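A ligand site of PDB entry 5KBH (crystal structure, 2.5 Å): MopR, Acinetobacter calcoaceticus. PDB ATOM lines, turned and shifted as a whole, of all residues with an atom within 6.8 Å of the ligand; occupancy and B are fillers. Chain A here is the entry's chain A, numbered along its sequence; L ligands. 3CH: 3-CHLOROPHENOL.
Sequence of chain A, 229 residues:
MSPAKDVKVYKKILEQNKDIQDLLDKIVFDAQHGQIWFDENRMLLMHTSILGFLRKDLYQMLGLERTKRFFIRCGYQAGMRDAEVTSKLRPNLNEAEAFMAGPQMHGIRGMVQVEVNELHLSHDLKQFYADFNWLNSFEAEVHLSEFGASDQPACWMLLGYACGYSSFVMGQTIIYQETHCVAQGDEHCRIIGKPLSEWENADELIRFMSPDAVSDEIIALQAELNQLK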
ATOM      1  N   GLY A  79       3.661  -3.298  -2.966  1.00  0.00           N
ATOM      2  CA  GLY A  79       2.818  -2.141  -3.333  1.00  0.00           C
ATOM      3  C   GLY A  79       3.066  -0.978  -2.432  1.00  0.00           C
ATOM      4  O   GLY A  79       3.192   0.160  -2.854  1.00  0.00           O
ATOM      5  N   PHE A  99      -1.492   9.220  -7.766  1.00  0.00           N
ATOM      6  CA  PHE A  99      -1.967   7.853  -7.577  1.00  0.00           C
ATOM      7  C   PHE A  99      -1.633   6.913  -8.725  1.00  0.00           C
ATOM      8  O   PHE A  99      -1.285   5.755  -8.507  1.00  0.00           O
ATOM      9  CB  PHE A  99      -3.489   7.826  -7.393  1.00  0.00           C
ATOM     10  CG  PHE A  99      -4.031   6.452  -7.186  1.00  0.00           C
ATOM     11  CD1 PHE A  99      -3.952   5.832  -5.945  1.00  0.00           C
ATOM     12  CD2 PHE A  99      -4.562   5.740  -8.246  1.00  0.00           C
ATOM     13  CE1 PHE A  99      -4.425   4.549  -5.758  1.00  0.00           C
ATOM     14  CE2 PHE A  99      -5.017   4.454  -8.083  1.00  0.00           C
ATOM     15  CZ  PHE A  99      -4.952   3.849  -6.834  1.00  0.00           C
ATOM     16  N   MET A 100      -1.740   7.410  -9.934  1.00  0.00           N
ATOM     17  CA  MET A 100      -1.555   6.586 -11.116  1.00  0.00           C
ATOM     18  C   MET A 100      -0.202   5.901 -11.256  1.00  0.00           C
ATOM     19  O   MET A 100      -0.068   4.998 -12.069  1.00  0.00           O
ATOM     20  CB  MET A 100      -1.862   7.396 -12.380  1.00  0.00           C
ATOM     21  CG  MET A 100      -3.346   7.583 -12.621  1.00  0.00           C
ATOM     22  SD  MET A 100      -4.074   5.955 -12.855  1.00  0.00           S
ATOM     23  CE  MET A 100      -5.564   6.214 -11.952  1.00  0.00           C
ATOM     24  N   ALA A 101       0.786   6.317 -10.476  1.00  0.00           N
ATOM     25  CA  ALA A 101       2.073   5.612 -10.431  1.00  0.00           C
ATOM     26  C   ALA A 101       1.916   4.109 -10.188  1.00  0.00           C
ATOM     27  O   ALA A 101       2.553   3.303 -10.856  1.00  0.00           O
ATOM     28  CB  ALA A 101       2.975   6.220  -9.357  1.00  0.00           C
ATOM     29  N   GLY A 102       1.039   3.732  -9.277  1.00  0.00           N
ATOM     30  CA  GLY A 102       0.853   2.323  -8.961  1.00  0.00           C
ATOM     31  C   GLY A 102       0.425   1.418 -10.137  1.00  0.00           C
ATOM     32  O   GLY A 102       1.049   0.370 -10.346  1.00  0.00           O
ATOM     33  N   PRO A 103      -0.649   1.788 -10.874  1.00  0.00           N
ATOM     34  CA  PRO A 103      -0.998   1.120 -12.152  1.00  0.00           C
ATOM     35  C   PRO A 103       0.094   1.191 -13.212  1.00  0.00           C
ATOM     36  O   PRO A 103       0.208   0.300 -14.045  1.00  0.00           O
ATOM     37  CB  PRO A 103      -2.238   1.881 -12.620  1.00  0.00           C
ATOM     38  CG  PRO A 103      -2.872   2.322 -11.352  1.00  0.00           C
ATOM     39  CD  PRO A 103      -1.770   2.629 -10.390  1.00  0.00           C
ATOM     40  N   GLN A 104       0.852   2.275 -13.197  1.00  0.00           N
ATOM     41  CA  GLN A 104       1.977   2.466 -14.102  1.00  0.00           C
ATOM     42  C   GLN A 104       3.146   1.538 -13.742  1.00  0.00           C
ATOM     43  O   GLN A 104       3.716   0.880 -14.617  1.00  0.00           O
ATOM     44  CB  GLN A 104       2.412   3.955 -14.126  1.00  0.00           C
ATOM     45  CG  GLN A 104       1.412   4.853 -14.845  1.00  0.00           C
ATOM     46  CD  GLN A 104       1.447   6.332 -14.471  1.00  0.00           C
ATOM     47  OE1 GLN A 104       2.250   6.792 -13.647  1.00  0.00           O
ATOM     48  NE2 GLN A 104       0.536   7.082 -15.079  1.00  0.00           N
ATOM     49  N   MET A 105       3.464   1.464 -12.451  1.00  0.00           N
ATOM     50  CA  MET A 105       4.471   0.513 -11.979  1.00  0.00           C
ATOM     51  C   MET A 105       4.116  -0.948 -12.243  1.00  0.00           C
ATOM     52  O   MET A 105       4.963  -1.748 -12.590  1.00  0.00           O
ATOM     53  CB  MET A 105       4.809   0.753 -10.509  1.00  0.00           C
ATOM     54  CG  MET A 105       5.562   2.074 -10.253  1.00  0.00           C
ATOM     55  SD  MET A 105       7.348   1.972 -10.512  1.00  0.00           S
ATOM     56  CE  MET A 105       7.498   1.846 -12.274  1.00  0.00           C
ATOM     57  N   HIS A 106       2.852  -1.307 -12.119  1.00  0.00           N
ATOM     58  CA  HIS A 106       2.436  -2.635 -12.474  1.00  0.00           C
ATOM     59  C   HIS A 106       2.703  -2.972 -13.915  1.00  0.00           C
ATOM     60  O   HIS A 106       3.091  -4.088 -14.232  1.00  0.00           O
ATOM     61  CB  HIS A 106       0.940  -2.857 -12.187  1.00  0.00           C
ATOM     62  CG  HIS A 106       0.680  -3.832 -11.080  1.00  0.00           C
ATOM     63  ND1 HIS A 106      -0.535  -3.935 -10.466  1.00  0.00           N
ATOM     64  CD2 HIS A 106       1.492  -4.735 -10.477  1.00  0.00           C
ATOM     65  CE1 HIS A 106      -0.483  -4.876  -9.545  1.00  0.00           C
ATOM     66  NE2 HIS A 106       0.738  -5.372  -9.528  1.00  0.00           N
ATOM     67  N   GLY A 107       2.448  -2.003 -14.795  1.00  0.00           N
ATOM     68  CA  GLY A 107       2.744  -2.177 -16.214  1.00  0.00           C
ATOM     69  C   GLY A 107       4.239  -2.154 -16.530  1.00  0.00           C
ATOM     70  O   GLY A 107       4.729  -3.001 -17.294  1.00  0.00           O
ATOM     71  N   VAL A 112       0.850  -6.500 -15.216  1.00  0.00           N
ATOM     72  CA  VAL A 112      -0.501  -6.301 -15.707  1.00  0.00           C
ATOM     73  C   VAL A 112      -0.622  -4.910 -16.285  1.00  0.00           C
ATOM     74  O   VAL A 112       0.076  -3.988 -15.862  1.00  0.00           O
ATOM     75  CB  VAL A 112      -1.566  -6.572 -14.622  1.00  0.00           C
ATOM     76  CG1 VAL A 112      -1.310  -5.760 -13.360  1.00  0.00           C
ATOM     77  CG2 VAL A 112      -2.969  -6.309 -15.141  1.00  0.00           C
ATOM     78  N   GLN A 113      -1.465  -4.800 -17.309  1.00  0.00           N
ATOM     79  CA  GLN A 113      -1.896  -3.532 -17.850  1.00  0.00           C
ATOM     80  C   GLN A 113      -3.192  -3.043 -17.180  1.00  0.00           C
ATOM     81  O   GLN A 113      -4.244  -3.714 -17.197  1.00  0.00           O
ATOM     82  CB  GLN A 113      -2.149  -3.724 -19.330  1.00  0.00           C
ATOM     83  CG  GLN A 113      -2.460  -2.435 -20.056  1.00  0.00           C
ATOM     84  CD  GLN A 113      -2.980  -2.659 -21.450  1.00  0.00           C
ATOM     85  OE1 GLN A 113      -2.867  -3.735 -22.055  1.00  0.00           O
ATOM     86  NE2 GLN A 113      -3.593  -1.615 -21.976  1.00  0.00           N
ATOM     87  N   VAL A 114      -3.132  -1.863 -16.590  1.00  0.00           N
ATOM     88  CA  VAL A 114      -4.315  -1.276 -15.976  1.00  0.00           C
ATOM     89  C   VAL A 114      -5.070  -0.333 -16.938  1.00  0.00           C
ATOM     90  O   VAL A 114      -4.461   0.527 -17.559  1.00  0.00           O
ATOM     91  CB  VAL A 114      -3.977  -0.594 -14.641  1.00  0.00           C
ATOM     92  CG1 VAL A 114      -5.189   0.172 -14.092  1.00  0.00           C
ATOM     93  CG2 VAL A 114      -3.493  -1.619 -13.631  1.00  0.00           C
ATOM     94  N   PHE A 128     -12.499   6.767  -1.358  1.00  0.00           N
ATOM     95  CA  PHE A 128     -11.837   6.062  -2.422  1.00  0.00           C
ATOM     96  C   PHE A 128     -12.778   5.065  -3.096  1.00  0.00           C
ATOM     97  O   PHE A 128     -13.538   4.357  -2.447  1.00  0.00           O
ATOM     98  CB  PHE A 128     -10.655   5.295  -1.859  1.00  0.00           C
ATOM     99  CG  PHE A 128      -9.732   4.740  -2.912  1.00  0.00           C
ATOM    100  CD1 PHE A 128      -9.989   3.508  -3.503  1.00  0.00           C
ATOM    101  CD2 PHE A 128      -8.602   5.458  -3.293  1.00  0.00           C
ATOM    102  CE1 PHE A 128      -9.130   3.010  -4.467  1.00  0.00           C
ATOM    103  CE2 PHE A 128      -7.741   4.962  -4.243  1.00  0.00           C
ATOM    104  CZ  PHE A 128      -7.998   3.730  -4.834  1.00  0.00           C
ATOM    105  N   ALA A 130     -12.303   2.620  -6.775  1.00  0.00           N
ATOM    106  CA  ALA A 130     -11.598   2.316  -8.018  1.00  0.00           C
ATOM    107  C   ALA A 130     -12.281   1.186  -8.722  1.00  0.00           C
ATOM    108  O   ALA A 130     -12.742   0.240  -8.107  1.00  0.00           O
ATOM    109  CB  ALA A 130     -10.164   1.948  -7.729  1.00  0.00           C
ATOM    110  N   PHE A 132     -11.080  -0.788 -12.057  1.00  0.00           N
ATOM    111  CA  PHE A 132     -10.058  -0.938 -13.090  1.00  0.00           C
ATOM    112  C   PHE A 132     -10.217  -2.274 -13.784  1.00  0.00           C
ATOM    113  O   PHE A 132     -10.727  -3.227 -13.197  1.00  0.00           O
ATOM    114  CB  PHE A 132      -8.659  -0.898 -12.481  1.00  0.00           C
ATOM    115  CG  PHE A 132      -8.318   0.331 -11.701  1.00  0.00           C
ATOM    116  CD1 PHE A 132      -8.964   1.552 -11.896  1.00  0.00           C
ATOM    117  CD2 PHE A 132      -7.257   0.298 -10.789  1.00  0.00           C
ATOM    118  CE1 PHE A 132      -8.596   2.682 -11.181  1.00  0.00           C
ATOM    119  CE2 PHE A 132      -6.875   1.437 -10.078  1.00  0.00           C
ATOM    120  CZ  PHE A 132      -7.544   2.629 -10.273  1.00  0.00           C
ATOM    121  N   TRP A 134      -7.869  -5.208 -15.768  1.00  0.00           N
ATOM    122  CA  TRP A 134      -6.532  -5.742 -15.742  1.00  0.00           C
ATOM    123  C   TRP A 134      -6.428  -6.550 -17.028  1.00  0.00           C
ATOM    124  O   TRP A 134      -7.176  -7.524 -17.187  1.00  0.00           O
ATOM    125  CB  TRP A 134      -6.331  -6.637 -14.510  1.00  0.00           C
ATOM    126  CG  TRP A 134      -5.784  -5.985 -13.252  1.00  0.00           C
ATOM    127  CD1 TRP A 134      -5.159  -4.775 -13.137  1.00  0.00           C
ATOM    128  CD2 TRP A 134      -5.734  -6.589 -11.944  1.00  0.00           C
ATOM    129  NE1 TRP A 134      -4.748  -4.559 -11.820  1.00  0.00           N
ATOM    130  CE2 TRP A 134      -5.087  -5.662 -11.068  1.00  0.00           C
ATOM    131  CE3 TRP A 134      -6.182  -7.816 -11.414  1.00  0.00           C
ATOM    132  CZ2 TRP A 134      -4.898  -5.927  -9.702  1.00  0.00           C
ATOM    133  CZ3 TRP A 134      -5.993  -8.077 -10.070  1.00  0.00           C
ATOM    134  CH2 TRP A 134      -5.374  -7.134  -9.213  1.00  0.00           C
ATOM    135  N   LEU A 158      -1.064  -9.637  -7.550  1.00  0.00           N
ATOM    136  CA  LEU A 158      -1.517  -8.358  -8.125  1.00  0.00           C
ATOM    137  C   LEU A 158      -2.495  -7.643  -7.217  1.00  0.00           C
ATOM    138  O   LEU A 158      -2.404  -6.421  -7.039  1.00  0.00           O
ATOM    139  CB  LEU A 158      -2.179  -8.536  -9.503  1.00  0.00           C
ATOM    140  CG  LEU A 158      -1.369  -9.187 -10.623  1.00  0.00           C
ATOM    141  CD1 LEU A 158      -2.095  -9.062 -11.960  1.00  0.00           C
ATOM    142  CD2 LEU A 158       0.025  -8.631 -10.730  1.00  0.00           C
ATOM    143  N   TYR A 161      -0.801  -6.123  -3.994  1.00  0.00           N
ATOM    144  CA  TYR A 161      -0.122  -4.932  -4.453  1.00  0.00           C
ATOM    145  C   TYR A 161      -1.091  -3.768  -4.580  1.00  0.00           C
ATOM    146  O   TYR A 161      -0.802  -2.663  -4.109  1.00  0.00           O
ATOM    147  CB  TYR A 161       0.563  -5.207  -5.803  1.00  0.00           C
ATOM    148  CG  TYR A 161       1.400  -4.062  -6.338  1.00  0.00           C
ATOM    149  CD1 TYR A 161       0.820  -3.040  -7.096  1.00  0.00           C
ATOM    150  CD2 TYR A 161       2.766  -3.991  -6.087  1.00  0.00           C
ATOM    151  CE1 TYR A 161       1.572  -1.982  -7.573  1.00  0.00           C
ATOM    152  CE2 TYR A 161       3.529  -2.955  -6.577  1.00  0.00           C
ATOM    153  CZ  TYR A 161       2.924  -1.944  -7.323  1.00  0.00           C
ATOM    154  OH  TYR A 161       3.641  -0.889  -7.809  1.00  0.00           O
ATOM    155  N   ALA A 162      -2.228  -4.005  -5.213  1.00  0.00           N
ATOM    156  CA  ALA A 162      -3.264  -2.956  -5.311  1.00  0.00           C
ATOM    157  C   ALA A 162      -3.678  -2.408  -3.936  1.00  0.00           C
ATOM    158  O   ALA A 162      -3.637  -1.208  -3.734  1.00  0.00           O
ATOM    159  CB  ALA A 162      -4.477  -3.441  -6.086  1.00  0.00           C
ATOM    160  N   CYS A 163      -4.028  -3.298  -2.998  1.00  0.00           N
ATOM    161  CA  CYS A 163      -4.351  -2.906  -1.591  1.00  0.00           C
ATOM    162  C   CYS A 163      -3.211  -2.173  -0.853  1.00  0.00           C
ATOM    163  O   CYS A 163      -3.456  -1.192  -0.169  1.00  0.00           O
ATOM    164  CB  CYS A 163      -4.726  -4.136  -0.763  1.00  0.00           C
ATOM    165  SG  CYS A 163      -6.081  -5.157  -1.438  1.00  0.00           S
ATOM    166  N   GLY A 164      -1.988  -2.679  -0.979  1.00  0.00           N
ATOM    167  CA  GLY A 164      -0.822  -2.091  -0.351  1.00  0.00           C
ATOM    168  C   GLY A 164      -0.497  -0.710  -0.908  1.00  0.00           C
ATOM    169  O   GLY A 164      -0.329   0.247  -0.145  1.00  0.00           O
ATOM    170  N   TYR A 165      -0.394  -0.612  -2.235  1.00  0.00           N
ATOM    171  CA  TYR A 165      -0.133   0.685  -2.852  1.00  0.00           C
ATOM    172  C   TYR A 165      -1.210   1.664  -2.411  1.00  0.00           C
ATOM    173  O   TYR A 165      -0.904   2.709  -1.843  1.00  0.00           O
ATOM    174  CB  TYR A 165      -0.060   0.606  -4.385  1.00  0.00           C
ATOM    175  CG  TYR A 165       0.156   1.980  -5.019  1.00  0.00           C
ATOM    176  CD1 TYR A 165      -0.926   2.849  -5.241  1.00  0.00           C
ATOM    177  CD2 TYR A 165       1.433   2.440  -5.343  1.00  0.00           C
ATOM    178  CE1 TYR A 165      -0.736   4.113  -5.772  1.00  0.00           C
ATOM    179  CE2 TYR A 165       1.637   3.712  -5.877  1.00  0.00           C
ATOM    180  CZ  TYR A 165       0.541   4.544  -6.079  1.00  0.00           C
ATOM    181  OH  TYR A 165       0.683   5.797  -6.602  1.00  0.00           O
ATOM    182  N   SER A 166      -2.459   1.300  -2.648  1.00  0.00           N
ATOM    183  CA  SER A 166      -3.586   2.178  -2.376  1.00  0.00           C
ATOM    184  C   SER A 166      -3.781   2.555  -0.929  1.00  0.00           C
ATOM    185  O   SER A 166      -4.109   3.689  -0.636  1.00  0.00           O
ATOM    186  CB  SER A 166      -4.870   1.574  -2.926  1.00  0.00           C
ATOM    187  OG  SER A 166      -4.761   1.399  -4.347  1.00  0.00           O
ATOM    188  N   TYR A 176      -9.437  -4.293  -2.209  1.00  0.00           N
ATOM    189  CA  TYR A 176      -9.921  -4.594  -3.564  1.00  0.00           C
ATOM    190  C   TYR A 176     -10.509  -5.998  -3.685  1.00  0.00           C
ATOM    191  O   TYR A 176     -10.120  -6.899  -2.955  1.00  0.00           O
ATOM    192  CB  TYR A 176      -8.772  -4.505  -4.562  1.00  0.00           C
ATOM    193  CG  TYR A 176      -8.293  -3.129  -4.868  1.00  0.00           C
ATOM    194  CD1 TYR A 176      -7.448  -2.454  -3.994  1.00  0.00           C
ATOM    195  CD2 TYR A 176      -8.608  -2.506  -6.068  1.00  0.00           C
ATOM    196  CE1 TYR A 176      -6.969  -1.184  -4.289  1.00  0.00           C
ATOM    197  CE2 TYR A 176      -8.142  -1.235  -6.389  1.00  0.00           C
ATOM    198  CZ  TYR A 176      -7.324  -0.577  -5.495  1.00  0.00           C
ATOM    199  OH  TYR A 176      -6.831   0.659  -5.824  1.00  0.00           O
ATOM    200  N   ILE A 191     -11.092  -5.373 -11.214  1.00  0.00           N
ATOM    201  CA  ILE A 191     -11.037  -5.119  -9.805  1.00  0.00           C
ATOM    202  C   ILE A 191     -11.894  -3.933  -9.347  1.00  0.00           C
ATOM    203  O   ILE A 191     -12.158  -2.987 -10.108  1.00  0.00           O
ATOM    204  CB  ILE A 191      -9.592  -4.945  -9.303  1.00  0.00           C
ATOM    205  CG1 ILE A 191      -8.881  -3.761  -9.960  1.00  0.00           C
ATOM    206  CG2 ILE A 191      -8.788  -6.209  -9.529  1.00  0.00           C
ATOM    207  CD1 ILE A 191      -7.561  -3.408  -9.294  1.00  0.00           C
HETATM  208  C4  3CH L   1      -3.697   0.233  -7.583  1.00  0.00           C
HETATM  209  C5  3CH L   1      -4.722  -0.469  -8.176  1.00  0.00           C
HETATM  210  C3  3CH L   1      -2.411  -0.002  -8.013  1.00  0.00           C
HETATM  211  C6  3CH L   1      -4.394  -1.383  -9.182  1.00  0.00           C
HETATM  212  C2  3CH L   1      -2.066  -0.886  -8.982  1.00  0.00           C
HETATM  213  C1  3CH L   1      -3.080  -1.590  -9.561  1.00  0.00           C
HETATM  214  OH  3CH L   1      -2.783  -2.480 -10.544  1.00  0.00           O
HETATM  215 CL   3CH L   1      -1.125   0.894  -7.279  1.00  0.00          CL
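An oxygen (OH) of the ligand is in hydrogen-bond range of a ring nitrogen (ND1) of His 106, 2.7 Å away.
NE1 of Trp 134 sits at hydrogen-bond distance from OH of the ligand, 3.1 Å away.
Phe 99 touches the ligand.
Gly 102 touches the ligand.
Pro 103 touches the ligand (N to C2, 3.6 Å).
Val 114 touches the ligand.
Phe 132 touches the ligand.
Tyr 161 touches the ligand.
Ala 162 touches the ligand (CB to C5, 3.6 Å).
Tyr 165 touches the ligand (CG to CL, 2.8 Å).
Ser 166 touches the ligand (OG to C4, 3.6 Å).
OH of Tyr 176 touches C5 of the ligand, 3.4 Å away.
CD1 of Ile 191 touches C6 of the ligand (3.8 Å).
Hydrophobic or aromatic side chains that line the ligand: Phe 99, Pro 103, His 106, Val 114, Phe 132, Trp 134, Tyr 161, Ala 162, Tyr 165, Tyr 176 and Ile 191.
The nearest printed residue that does not touch the ligand is Val 112 (4.6 Å).
The backbone carbonyl oxygen (O) of His 106 lies within hydrogen-bond range of the backbone NH (N) of Val 112 (3.4 Å).
The backbone NH (N) of Gly 102 lies close to the side-chain hydroxyl (OH) of Tyr 165, at 3.4 Å.
OH of Tyr 165 sits at hydrogen-bond distance from O of Phe 99 (2.7 Å).
The side-chain hydroxyl of Ser 166 sits at hydrogen-bond distance from the side-chain hydroxyl of Tyr 176 (2.6 Å).
N of Tyr 176 is in hydrogen-bond range of SG of Cys 163 (3.6 Å).
The backbone carbonyl oxygen (O) of Phe 132 lies within hydrogen-bond range of the backbone NH (N) of Ile 191 (2.9 Å).
OG of Ser 166 sits at hydrogen-bond distance from O of Ala 162, 2.9 Å away.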
